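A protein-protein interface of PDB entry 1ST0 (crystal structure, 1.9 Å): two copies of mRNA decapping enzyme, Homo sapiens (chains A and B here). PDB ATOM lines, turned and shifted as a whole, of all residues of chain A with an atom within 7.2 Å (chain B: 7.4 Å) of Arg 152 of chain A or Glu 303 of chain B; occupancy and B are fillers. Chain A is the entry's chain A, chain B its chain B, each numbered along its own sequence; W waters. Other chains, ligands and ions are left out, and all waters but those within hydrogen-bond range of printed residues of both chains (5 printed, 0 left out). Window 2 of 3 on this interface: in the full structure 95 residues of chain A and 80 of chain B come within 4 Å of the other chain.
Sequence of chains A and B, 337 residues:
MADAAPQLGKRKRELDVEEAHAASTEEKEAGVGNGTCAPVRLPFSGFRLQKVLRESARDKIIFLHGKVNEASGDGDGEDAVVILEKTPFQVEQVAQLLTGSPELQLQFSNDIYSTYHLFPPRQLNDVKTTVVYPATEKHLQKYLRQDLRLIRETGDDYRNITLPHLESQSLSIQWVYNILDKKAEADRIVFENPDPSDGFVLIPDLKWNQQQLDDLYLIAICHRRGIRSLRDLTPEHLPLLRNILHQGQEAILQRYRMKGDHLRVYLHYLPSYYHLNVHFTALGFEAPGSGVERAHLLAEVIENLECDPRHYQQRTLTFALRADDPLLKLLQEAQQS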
ATOM      1  N   LEU A 150       2.532   6.727   9.050  1.00  0.00           N
ATOM      2  CA  LEU A 150       2.060   7.268  10.340  1.00  0.00           C
ATOM      3  C   LEU A 150       0.552   7.546  10.354  1.00  0.00           C
ATOM      4  O   LEU A 150      -0.029   7.948   9.376  1.00  0.00           O
ATOM      5  CB  LEU A 150       2.817   8.563  10.684  1.00  0.00           C
ATOM      6  CG  LEU A 150       3.543   8.821  12.024  1.00  0.00           C
ATOM      7  CD1 LEU A 150       4.021   7.536  12.827  1.00  0.00           C
ATOM      8  CD2 LEU A 150       4.763   9.737  11.839  1.00  0.00           C
ATOM      9  N   ILE A 151      -0.099   7.349  11.474  1.00  0.00           N
ATOM     10  CA  ILE A 151      -1.460   7.720  11.580  1.00  0.00           C
ATOM     11  C   ILE A 151      -1.577   8.340  12.943  1.00  0.00           C
ATOM     12  O   ILE A 151      -0.855   7.939  13.877  1.00  0.00           O
ATOM     13  CB  ILE A 151      -2.400   6.488  11.384  1.00  0.00           C
ATOM     14  CG1 ILE A 151      -3.827   6.964  11.172  1.00  0.00           C
ATOM     15  CG2 ILE A 151      -2.390   5.568  12.608  1.00  0.00           C
ATOM     16  CD1 ILE A 151      -3.965   7.753   9.879  1.00  0.00           C
ATOM     17  N   ARG A 152      -2.421   9.354  13.069  1.00  0.00           N
ATOM     18  CA  ARG A 152      -2.677   9.934  14.382  1.00  0.00           C
ATOM     19  C   ARG A 152      -4.082   9.544  14.750  1.00  0.00           C
ATOM     20  O   ARG A 152      -5.045   9.961  14.102  1.00  0.00           O
ATOM     21  CB  ARG A 152      -2.438  11.470  14.398  1.00  0.00           C
ATOM     22  CG  ARG A 152      -1.131  11.933  13.756  1.00  0.00           C
ATOM     23  CD  ARG A 152      -0.577  13.313  14.215  1.00  0.00           C
ATOM     24  NE  ARG A 152      -0.374  13.415  15.659  1.00  0.00           N
ATOM     25  CZ  ARG A 152      -1.063  14.212  16.463  1.00  0.00           C
ATOM     26  NH1 ARG A 152      -2.015  14.990  15.969  1.00  0.00           N
ATOM     27  NH2 ARG A 152      -0.833  14.224  17.782  1.00  0.00           N
ATOM     28  N   GLU A 153      -4.212   8.739  15.787  1.00  0.00           N
ATOM     29  CA  GLU A 153      -5.464   8.165  16.225  1.00  0.00           C
ATOM     30  C   GLU A 153      -6.105   8.944  17.383  1.00  0.00           C
ATOM     31  O   GLU A 153      -5.606   8.892  18.520  1.00  0.00           O
ATOM     32  CB  GLU A 153      -5.201   6.699  16.624  1.00  0.00           C
ATOM     33  CG  GLU A 153      -6.427   5.926  17.019  1.00  0.00           C
ATOM     34  CD  GLU A 153      -6.119   4.723  17.912  1.00  0.00           C
ATOM     35  OE1 GLU A 153      -6.388   3.607  17.465  1.00  0.00           O
ATOM     36  OE2 GLU A 153      -5.674   4.907  19.060  1.00  0.00           O
ATOM     37  N   THR A 154      -7.211   9.668  17.111  1.00  0.00           N
ATOM     38  CA  THR A 154      -7.916  10.420  18.127  1.00  0.00           C
ATOM     39  C   THR A 154      -8.608   9.450  19.057  1.00  0.00           C
ATOM     40  O   THR A 154      -8.769   8.274  18.739  1.00  0.00           O
ATOM     41  CB  THR A 154      -8.994  11.359  17.453  1.00  0.00           C
ATOM     42  OG1 THR A 154     -10.075  10.541  16.976  1.00  0.00           O
ATOM     43  CG2 THR A 154      -8.408  11.989  16.170  1.00  0.00           C
ATOM     44  N   ASP A 157     -11.482   8.000  17.085  1.00  0.00           N
ATOM     45  CA  ASP A 157     -11.021   6.997  16.140  1.00  0.00           C
ATOM     46  C   ASP A 157     -10.861   5.676  16.844  1.00  0.00           C
ATOM     47  O   ASP A 157     -11.220   4.629  16.305  1.00  0.00           O
ATOM     48  CB  ASP A 157      -9.664   7.352  15.530  1.00  0.00           C
ATOM     49  CG  ASP A 157      -9.735   8.528  14.595  1.00  0.00           C
ATOM     50  OD1 ASP A 157     -10.859   8.814  14.097  1.00  0.00           O
ATOM     51  OD2 ASP A 157      -8.725   9.220  14.305  1.00  0.00           O
ATOM     52  N   ARG A 231      -4.524   2.414  25.935  1.00  0.00           N
ATOM     53  CA  ARG A 231      -5.886   2.990  25.899  1.00  0.00           C
ATOM     54  C   ARG A 231      -6.771   2.579  27.081  1.00  0.00           C
ATOM     55  O   ARG A 231      -7.695   3.337  27.419  1.00  0.00           O
ATOM     56  CB  ARG A 231      -6.588   2.787  24.530  1.00  0.00           C
ATOM     57  CG  ARG A 231      -5.696   3.266  23.314  1.00  0.00           C
ATOM     58  CD  ARG A 231      -6.194   4.277  22.235  1.00  0.00           C
ATOM     59  NE  ARG A 231      -6.367   5.591  22.750  1.00  0.00           N
ATOM     60  CZ  ARG A 231      -6.225   6.763  22.133  1.00  0.00           C
ATOM     61  NH1 ARG A 231      -5.820   6.951  20.872  1.00  0.00           N
ATOM     62  NH2 ARG A 231      -6.470   7.806  22.891  1.00  0.00           N
ATOM     63  N   ARG A 315      -6.831  11.688  24.497  1.00  0.00           N
ATOM     64  CA  ARG A 315      -5.805  12.187  23.609  1.00  0.00           C
ATOM     65  C   ARG A 315      -5.509  11.382  22.382  1.00  0.00           C
ATOM     66  O   ARG A 315      -5.829  10.188  22.282  1.00  0.00           O
ATOM     67  CB  ARG A 315      -4.527  12.454  24.412  1.00  0.00           C
ATOM     68  CG  ARG A 315      -4.675  13.725  25.277  1.00  0.00           C
ATOM     69  CD  ARG A 315      -4.328  14.999  24.507  1.00  0.00           C
ATOM     70  NE  ARG A 315      -3.377  15.684  25.331  1.00  0.00           N
ATOM     71  CZ  ARG A 315      -2.156  15.997  24.987  1.00  0.00           C
ATOM     72  NH1 ARG A 315      -1.685  15.764  23.772  1.00  0.00           N
ATOM     73  NH2 ARG A 315      -1.409  16.576  25.898  1.00  0.00           N
ATOM     74  N   THR A 316      -4.825  12.026  21.465  1.00  0.00           N
ATOM     75  CA  THR A 316      -4.469  11.457  20.196  1.00  0.00           C
ATOM     76  C   THR A 316      -3.089  10.770  20.285  1.00  0.00           C
ATOM     77  O   THR A 316      -2.146  11.370  20.738  1.00  0.00           O
ATOM     78  CB  THR A 316      -4.465  12.604  19.150  1.00  0.00           C
ATOM     79  OG1 THR A 316      -5.810  13.151  19.058  1.00  0.00           O
ATOM     80  CG2 THR A 316      -4.167  12.088  17.780  1.00  0.00           C
ATOM     81  N   LEU A 317      -3.010   9.514  19.853  1.00  0.00           N
ATOM     82  CA  LEU A 317      -1.771   8.737  19.903  1.00  0.00           C
ATOM     83  C   LEU A 317      -1.305   8.488  18.494  1.00  0.00           C
ATOM     84  O   LEU A 317      -2.136   8.224  17.586  1.00  0.00           O
ATOM     85  CB  LEU A 317      -2.012   7.406  20.637  1.00  0.00           C
ATOM     86  CG  LEU A 317      -2.505   7.485  22.091  1.00  0.00           C
ATOM     87  CD1 LEU A 317      -2.806   6.099  22.715  1.00  0.00           C
ATOM     88  CD2 LEU A 317      -1.474   8.204  22.926  1.00  0.00           C
ATOM     89  N   THR A 318      -0.006   8.591  18.275  1.00  0.00           N
ATOM     90  CA  THR A 318       0.553   8.444  16.936  1.00  0.00           C
ATOM     91  C   THR A 318       1.319   7.136  16.801  1.00  0.00           C
ATOM     92  O   THR A 318       2.188   6.839  17.634  1.00  0.00           O
ATOM     93  CB  THR A 318       1.515   9.630  16.704  1.00  0.00           C
ATOM     94  OG1 THR A 318       0.799  10.871  16.851  1.00  0.00           O
ATOM     95  CG2 THR A 318       2.074   9.652  15.343  1.00  0.00           C
ATOM     96  N   PHE A 319       1.074   6.392  15.725  1.00  0.00           N
ATOM     97  CA  PHE A 319       1.813   5.174  15.457  1.00  0.00           C
ATOM     98  C   PHE A 319       1.871   4.848  14.002  1.00  0.00           C
ATOM     99  O   PHE A 319       1.187   5.505  13.202  1.00  0.00           O
ATOM    100  CB  PHE A 319       1.174   4.000  16.226  1.00  0.00           C
ATOM    101  CG  PHE A 319      -0.305   3.847  15.989  1.00  0.00           C
ATOM    102  CD1 PHE A 319      -0.792   3.017  14.968  1.00  0.00           C
ATOM    103  CD2 PHE A 319      -1.200   4.506  16.807  1.00  0.00           C
ATOM    104  CE1 PHE A 319      -2.158   2.865  14.782  1.00  0.00           C
ATOM    105  CE2 PHE A 319      -2.570   4.329  16.638  1.00  0.00           C
ATOM    106  CZ  PHE A 319      -3.052   3.514  15.620  1.00  0.00           C
ATOM    107  N   LEU A 328      -5.444   1.040   8.669  1.00  0.00           N
ATOM    108  CA  LEU A 328      -4.965   2.313   8.137  1.00  0.00           C
ATOM    109  C   LEU A 328      -6.021   2.968   7.213  1.00  0.00           C
ATOM    110  O   LEU A 328      -6.426   4.143   7.444  1.00  0.00           O
ATOM    111  CB  LEU A 328      -3.655   2.102   7.348  1.00  0.00           C
ATOM    112  CG  LEU A 328      -3.005   3.403   6.833  1.00  0.00           C
ATOM    113  CD1 LEU A 328      -2.673   4.422   7.955  1.00  0.00           C
ATOM    114  CD2 LEU A 328      -1.781   3.106   6.083  1.00  0.00           C
ATOM    115  N   LEU A 331      -8.796   4.185   9.092  1.00  0.00           N
ATOM    116  CA  LEU A 331      -8.555   5.357   9.925  1.00  0.00           C
ATOM    117  C   LEU A 331      -8.463   6.589   9.024  1.00  0.00           C
ATOM    118  O   LEU A 331      -9.031   7.633   9.323  1.00  0.00           O
ATOM    119  CB  LEU A 331      -7.295   5.181  10.791  1.00  0.00           C
ATOM    120  CG  LEU A 331      -7.444   4.193  11.954  1.00  0.00           C
ATOM    121  CD1 LEU A 331      -6.102   3.854  12.535  1.00  0.00           C
ATOM    122  CD2 LEU A 331      -8.349   4.802  13.014  1.00  0.00           C
ATOM    123  N   GLN A 335     -10.944  10.162   8.670  1.00  0.00           N
ATOM    124  CA  GLN A 335     -10.234  11.407   8.964  1.00  0.00           C
ATOM    125  C   GLN A 335     -10.526  12.530   7.942  1.00  0.00           C
ATOM    126  O   GLN A 335      -9.916  13.610   7.980  1.00  0.00           O
ATOM    127  CB  GLN A 335      -8.734  11.159   9.200  1.00  0.00           C
ATOM    128  CG  GLN A 335      -8.487  10.319  10.481  1.00  0.00           C
ATOM    129  CD  GLN A 335      -7.046  10.307  10.964  1.00  0.00           C
ATOM    130  OE1 GLN A 335      -6.100  10.398  10.167  1.00  0.00           O
ATOM    131  NE2 GLN A 335      -6.879  10.202  12.278  1.00  0.00           N
ATOM    132  N   LEU B 238       2.834  28.627  19.127  1.00  0.00           N
ATOM    133  CA  LEU B 238       1.977  27.756  18.334  1.00  0.00           C
ATOM    134  C   LEU B 238       1.971  28.117  16.847  1.00  0.00           C
ATOM    135  O   LEU B 238       2.147  27.224  15.987  1.00  0.00           O
ATOM    136  CB  LEU B 238       0.585  27.696  18.934  1.00  0.00           C
ATOM    137  CG  LEU B 238       0.350  26.811  20.166  1.00  0.00           C
ATOM    138  CD1 LEU B 238      -0.955  27.113  20.846  1.00  0.00           C
ATOM    139  CD2 LEU B 238       0.390  25.283  19.755  1.00  0.00           C
ATOM    140  N   ARG B 242       3.336  25.124  14.215  1.00  0.00           N
ATOM    141  CA  ARG B 242       2.415  24.776  13.129  1.00  0.00           C
ATOM    142  C   ARG B 242       2.974  25.079  11.769  1.00  0.00           C
ATOM    143  O   ARG B 242       2.765  24.301  10.835  1.00  0.00           O
ATOM    144  CB  ARG B 242       1.072  25.480  13.251  1.00  0.00           C
ATOM    145  CG  ARG B 242       0.249  24.994  14.388  1.00  0.00           C
ATOM    146  CD  ARG B 242      -0.872  25.946  14.754  1.00  0.00           C
ATOM    147  NE  ARG B 242      -1.709  25.445  15.823  1.00  0.00           N
ATOM    148  CZ  ARG B 242      -2.455  26.220  16.582  1.00  0.00           C
ATOM    149  NH1 ARG B 242      -2.447  27.542  16.377  1.00  0.00           N
ATOM    150  NH2 ARG B 242      -3.208  25.692  17.540  1.00  0.00           N
ATOM    151  N   LEU B 245       5.758  22.437  10.986  1.00  0.00           N
ATOM    152  CA  LEU B 245       5.089  21.129  10.727  1.00  0.00           C
ATOM    153  C   LEU B 245       4.430  21.131   9.356  1.00  0.00           C
ATOM    154  O   LEU B 245       4.715  20.280   8.482  1.00  0.00           O
ATOM    155  CB  LEU B 245       4.016  20.887  11.771  1.00  0.00           C
ATOM    156  CG  LEU B 245       3.687  19.422  12.242  1.00  0.00           C
ATOM    157  CD1 LEU B 245       2.234  19.155  12.434  1.00  0.00           C
ATOM    158  CD2 LEU B 245       4.385  18.242  11.503  1.00  0.00           C
ATOM    159  N   LEU B 297       7.556  14.279  19.422  1.00  0.00           N
ATOM    160  CA  LEU B 297       6.974  14.488  18.103  1.00  0.00           C
ATOM    161  C   LEU B 297       6.436  15.951  18.066  1.00  0.00           C
ATOM    162  O   LEU B 297       5.789  16.358  18.971  1.00  0.00           O
ATOM    163  CB  LEU B 297       5.836  13.503  17.842  1.00  0.00           C
ATOM    164  CG  LEU B 297       6.336  12.090  17.477  1.00  0.00           C
ATOM    165  CD1 LEU B 297       5.090  11.220  17.740  1.00  0.00           C
ATOM    166  CD2 LEU B 297       6.919  11.962  16.035  1.00  0.00           C
ATOM    167  N   LEU B 298       6.707  16.670  17.024  1.00  0.00           N
ATOM    168  CA  LEU B 298       6.167  18.058  16.878  1.00  0.00           C
ATOM    169  C   LEU B 298       4.658  18.165  16.994  1.00  0.00           C
ATOM    170  O   LEU B 298       4.131  19.040  17.742  1.00  0.00           O
ATOM    171  CB  LEU B 298       6.627  18.649  15.565  1.00  0.00           C
ATOM    172  CG  LEU B 298       6.940  20.185  15.558  1.00  0.00           C
ATOM    173  CD1 LEU B 298       6.997  20.785  14.201  1.00  0.00           C
ATOM    174  CD2 LEU B 298       6.181  21.034  16.599  1.00  0.00           C
ATOM    175  N   ALA B 299       3.919  17.272  16.319  1.00  0.00           N
ATOM    176  CA  ALA B 299       2.454  17.332  16.435  1.00  0.00           C
ATOM    177  C   ALA B 299       1.969  17.187  17.830  1.00  0.00           C
ATOM    178  O   ALA B 299       0.951  17.798  18.212  1.00  0.00           O
ATOM    179  CB  ALA B 299       1.758  16.257  15.528  1.00  0.00           C
ATOM    180  N   GLU B 300       2.632  16.344  18.638  1.00  0.00           N
ATOM    181  CA  GLU B 300       2.198  16.201  20.039  1.00  0.00           C
ATOM    182  C   GLU B 300       2.608  17.377  20.882  1.00  0.00           C
ATOM    183  O   GLU B 300       1.934  17.676  21.834  1.00  0.00           O
ATOM    184  CB  GLU B 300       2.745  14.896  20.717  1.00  0.00           C
ATOM    185  CG  GLU B 300       2.061  13.664  20.182  1.00  0.00           C
ATOM    186  CD  GLU B 300       2.535  12.342  20.861  1.00  0.00           C
ATOM    187  OE1 GLU B 300       1.723  11.416  21.027  1.00  0.00           O
ATOM    188  OE2 GLU B 300       3.719  12.227  21.219  1.00  0.00           O
ATOM    189  N   VAL B 301       3.742  17.973  20.616  1.00  0.00           N
ATOM    190  CA  VAL B 301       4.180  19.149  21.360  1.00  0.00           C
ATOM    191  C   VAL B 301       3.103  20.268  21.151  1.00  0.00           C
ATOM    192  O   VAL B 301       2.685  20.893  22.084  1.00  0.00           O
ATOM    193  CB  VAL B 301       5.523  19.679  20.790  1.00  0.00           C
ATOM    194  CG1 VAL B 301       5.854  21.101  21.424  1.00  0.00           C
ATOM    195  CG2 VAL B 301       6.731  18.689  21.088  1.00  0.00           C
ATOM    196  N   ILE B 302       2.684  20.463  19.914  1.00  0.00           N
ATOM    197  CA  ILE B 302       1.594  21.388  19.611  1.00  0.00           C
ATOM    198  C   ILE B 302       0.346  21.053  20.416  1.00  0.00           C
ATOM    199  O   ILE B 302      -0.216  21.939  21.080  1.00  0.00           O
ATOM    200  CB  ILE B 302       1.324  21.363  18.101  1.00  0.00           C
ATOM    201  CG1 ILE B 302       2.474  22.060  17.410  1.00  0.00           C
ATOM    202  CG2 ILE B 302      -0.055  21.988  17.777  1.00  0.00           C
ATOM    203  CD1 ILE B 302       2.548  21.762  15.926  1.00  0.00           C
ATOM    204  N   GLU B 303      -0.070  19.792  20.422  1.00  0.00           N
ATOM    205  CA  GLU B 303      -1.289  19.443  21.164  1.00  0.00           C
ATOM    206  C   GLU B 303      -1.192  19.594  22.665  1.00  0.00           C
ATOM    207  O   GLU B 303      -2.192  19.926  23.322  1.00  0.00           O
ATOM    208  CB  GLU B 303      -1.842  18.044  20.783  1.00  0.00           C
ATOM    209  CG  GLU B 303      -2.502  18.052  19.409  1.00  0.00           C
ATOM    210  CD  GLU B 303      -2.869  16.656  18.874  1.00  0.00           C
ATOM    211  OE1 GLU B 303      -2.886  15.665  19.648  1.00  0.00           O
ATOM    212  OE2 GLU B 303      -3.157  16.558  17.677  1.00  0.00           O
ATOM    213  N   ASN B 304      -0.019  19.323  23.215  1.00  0.00           N
ATOM    214  CA  ASN B 304       0.252  19.585  24.636  1.00  0.00           C
ATOM    215  C   ASN B 304       0.076  21.088  25.012  1.00  0.00           C
ATOM    216  O   ASN B 304      -0.484  21.437  26.070  1.00  0.00           O
ATOM    217  CB  ASN B 304       1.686  19.111  25.000  1.00  0.00           C
ATOM    218  CG  ASN B 304       1.781  17.552  25.126  1.00  0.00           C
ATOM    219  OD1 ASN B 304       0.766  16.881  25.166  1.00  0.00           O
ATOM    220  ND2 ASN B 304       2.984  17.020  25.224  1.00  0.00           N
ATOM    221  N   LEU B 305       0.557  21.952  24.168  1.00  0.00           N
ATOM    222  CA  LEU B 305       0.366  23.383  24.402  1.00  0.00           C
ATOM    223  C   LEU B 305      -1.124  23.741  24.364  1.00  0.00           C
ATOM    224  O   LEU B 305      -1.604  24.501  25.238  1.00  0.00           O
ATOM    225  CB  LEU B 305       1.120  24.158  23.344  1.00  0.00           C
ATOM    226  CG  LEU B 305       2.610  24.011  23.470  1.00  0.00           C
ATOM    227  CD1 LEU B 305       3.239  24.537  22.211  1.00  0.00           C
ATOM    228  CD2 LEU B 305       3.153  24.741  24.724  1.00  0.00           C
ATOM    229  N   GLU B 306      -1.870  23.111  23.448  1.00  0.00           N
ATOM    230  CA  GLU B 306      -3.276  23.430  23.293  1.00  0.00           C
ATOM    231  C   GLU B 306      -3.987  22.971  24.509  1.00  0.00           C
ATOM    232  O   GLU B 306      -4.974  23.573  24.900  1.00  0.00           O
ATOM    233  CB  GLU B 306      -3.846  22.771  22.040  1.00  0.00           C
ATOM    234  CG  GLU B 306      -3.222  23.341  20.751  1.00  0.00           C
ATOM    235  CD  GLU B 306      -3.672  22.618  19.470  1.00  0.00           C
ATOM    236  OE1 GLU B 306      -4.480  21.662  19.546  1.00  0.00           O
ATOM    237  OE2 GLU B 306      -3.211  23.009  18.358  1.00  0.00           O
ATOM    238  N   CYS B 307      -3.454  21.936  25.169  1.00  0.00           N
ATOM    239  CA  CYS B 307      -4.153  21.328  26.289  1.00  0.00           C
ATOM    240  C   CYS B 307      -3.664  21.754  27.634  1.00  0.00           C
ATOM    241  O   CYS B 307      -4.341  21.555  28.642  1.00  0.00           O
ATOM    242  CB  CYS B 307      -4.039  19.783  26.216  1.00  0.00           C
ATOM    243  SG  CYS B 307      -5.343  19.146  25.195  1.00  0.00           S
ATOM    244  N   ASP B 308      -2.454  22.274  27.674  1.00  0.00           N
ATOM    245  CA  ASP B 308      -1.737  22.392  28.945  1.00  0.00           C
ATOM    246  C   ASP B 308      -0.722  23.490  28.681  1.00  0.00           C
ATOM    247  O   ASP B 308       0.449  23.207  28.435  1.00  0.00           O
ATOM    248  CB  ASP B 308      -1.104  21.019  29.288  1.00  0.00           C
ATOM    249  CG  ASP B 308      -0.272  21.017  30.589  1.00  0.00           C
ATOM    250  OD1 ASP B 308      -0.410  21.929  31.459  1.00  0.00           O
ATOM    251  OD2 ASP B 308       0.551  20.085  30.830  1.00  0.00           O
ATOM    252  N   PRO B 309      -1.182  24.768  28.709  1.00  0.00           N
ATOM    253  CA  PRO B 309      -0.334  25.918  28.310  1.00  0.00           C
ATOM    254  C   PRO B 309       1.103  25.974  28.869  1.00  0.00           C
ATOM    255  O   PRO B 309       2.053  26.295  28.149  1.00  0.00           O
ATOM    256  CB  PRO B 309      -1.146  27.162  28.772  1.00  0.00           C
ATOM    257  CG  PRO B 309      -2.562  26.689  28.870  1.00  0.00           C
ATOM    258  CD  PRO B 309      -2.551  25.181  29.105  1.00  0.00           C
ATOM    259  N   TYR B 312       5.556  22.534  29.254  1.00  0.00           N
ATOM    260  CA  TYR B 312       6.968  22.416  29.130  1.00  0.00           C
ATOM    261  C   TYR B 312       7.822  23.199  30.115  1.00  0.00           C
ATOM    262  O   TYR B 312       9.036  23.089  30.053  1.00  0.00           O
ATOM    263  CB  TYR B 312       7.379  22.721  27.700  1.00  0.00           C
ATOM    264  CG  TYR B 312       6.875  21.607  26.811  1.00  0.00           C
ATOM    265  CD1 TYR B 312       5.726  21.787  26.038  1.00  0.00           C
ATOM    266  CD2 TYR B 312       7.516  20.350  26.802  1.00  0.00           C
ATOM    267  CE1 TYR B 312       5.215  20.765  25.230  1.00  0.00           C
ATOM    268  CE2 TYR B 312       7.016  19.302  26.006  1.00  0.00           C
ATOM    269  CZ  TYR B 312       5.865  19.524  25.205  1.00  0.00           C
ATOM    270  OH  TYR B 312       5.322  18.534  24.416  1.00  0.00           O
HETATM  271  O   HOH W   1      -4.489  14.789  21.559  1.00  0.00           O
HETATM  272  O   HOH W   2       1.832   8.983  20.527  1.00  0.00           O
HETATM  273  O   HOH W   3      -1.381  14.503  21.570  1.00  0.00           O
HETATM  274  O   HOH W   4      -5.571  15.168  17.199  1.00  0.00           O
HETATM  275  O   HOH W   5       0.145  11.854  19.107  1.00  0.00           O
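OE2 of Glu 303 of chain B is in salt-bridge range of NH1 of Arg 152 of chain A (2.6 Å). OD1 of Asn 304 of chain B lies within hydrogen-bond range of NH1 of Arg 315 of chain A, 3.0 Å away.
The backbone carbonyl oxygen (O) of Glu 303 of chain B sits close to the side-chain sulfur (SG) of Cys 307 of chain B, 3.7 Å away. The side-chain hydroxyl (OH) of Tyr 312 of chain B is in hydrogen-bond range of the side-chain amide nitrogen (ND2) of Asn 304 of chain B. The guanidinium group (NE) of Arg 152 of chain A is in hydrogen-bond range of the side-chain hydroxyl (OG1) of Thr 318 of chain A (3.0 Å). The backbone carbonyl oxygen (O) of Arg 152 of chain A is in hydrogen-bond range of the side-chain amide nitrogen (NE2) of Gln 335 of chain A (2.6 Å). NH2 of Arg 231 of chain A sits at hydrogen-bond distance from O of Arg 315 of chain A (2.5 Å).
Arg 152 of chain A touches Ala 299 of chain B (NE to CB, 3.6 Å). NH2 of Arg 152 of chain A touches CG of Glu 300 of chain B, 3.8 Å away. Arg 315 of chain A touches Glu 303 of chain B. Arg 315 of chain A touches Cys 307 of chain B. Glu 300 of chain B touches Thr 316 of chain A (OE1 to O, 3.9 Å). Thr 316 of chain A touches Glu 303 of chain B.
Of chain B, only Ala 299, Glu 300 and Glu 303 come within 4 Å of Arg 152 of chain A. Of the printed residues of chain B, Arg 315 of chain A touches Glu 303 (3.8 Å), Asn 304 (2.3 Å) and Cys 307 (3.98 Å). Printed residues of chain B within 4 Å of Thr 316 of chain A: Glu 300 (3.9 Å) and Glu 303 (3.5 Å). Leu 245 of chain B touches none of the printed residues of chain A. Of the printed residues of chain A, Ala 299 of chain B touches Arg 152 (3.6 Å). Glu 303 of chain B touches just these residues of chain A: Arg 152 (2.6 Å), Arg 315 (3.8 Å) and Thr 316 (3.5 Å). Printed residues of chain A within 4 Å of Asn 304 of chain B: Arg 315. Of the printed residues of chain A, Cys 307 of chain B touches Arg 315. The nearest printed residue of chain A that does not touch Cys 307 of chain B is Thr 316 of chain A (8.1 Å).
Of the 15 printed residues of chain A, 3 touch a printed residue of chain B. Printed residues of chain A that touch a printed residue of chain B: Arg 152, Arg 315 and Thr 316. Among the printed residues, 8 pairs touch across the chains. Among the printed residues, Asp or Glu carboxylates within 4 Å of a Lys or Arg side-chain nitrogen of the other chain: Arg 152 of chain A with Glu 303 of chain B (2.6 Å).
No position is printed for both chains. Of the 8 pairs that touch across the chains among the printed residues, none has its exchanged pair printed and touching as well.
Water W2 bridges OE1 of Glu 300 of chain B and N of Thr 318 of chain A. Water W5 lies within hydrogen-bond range of the side-chain carboxylate (OE1) of Glu 300 of chain B (2.5 Å), the side-chain hydroxyl (OG1) of Thr 318 of chain A (2.5 Å), the backbone carbonyl oxygen (O) of Thr 316 of chain A (2.9 Å) and the guanidinium group (NH2) of Arg 152 of chain A (2.9 Å). Water W3 lies within hydrogen-bond range of NH1 of Arg 315 of chain A (2.6 Å), OE1 of Glu 303 of chain B (2.7 Å) and O of Thr 316 of chain A (3.3 Å). Water W1 lies within hydrogen-bond range of the side-chain carboxylate of Glu 303 of chain B (2.6 Å) and the backbone NH of Thr 316 of chain A (2.8 Å). Water W4 lies within hydrogen-bond range of OG1 of Thr 316 of chain A (2.8 Å) and OE2 of Glu 303 of chain B (2.8 Å).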
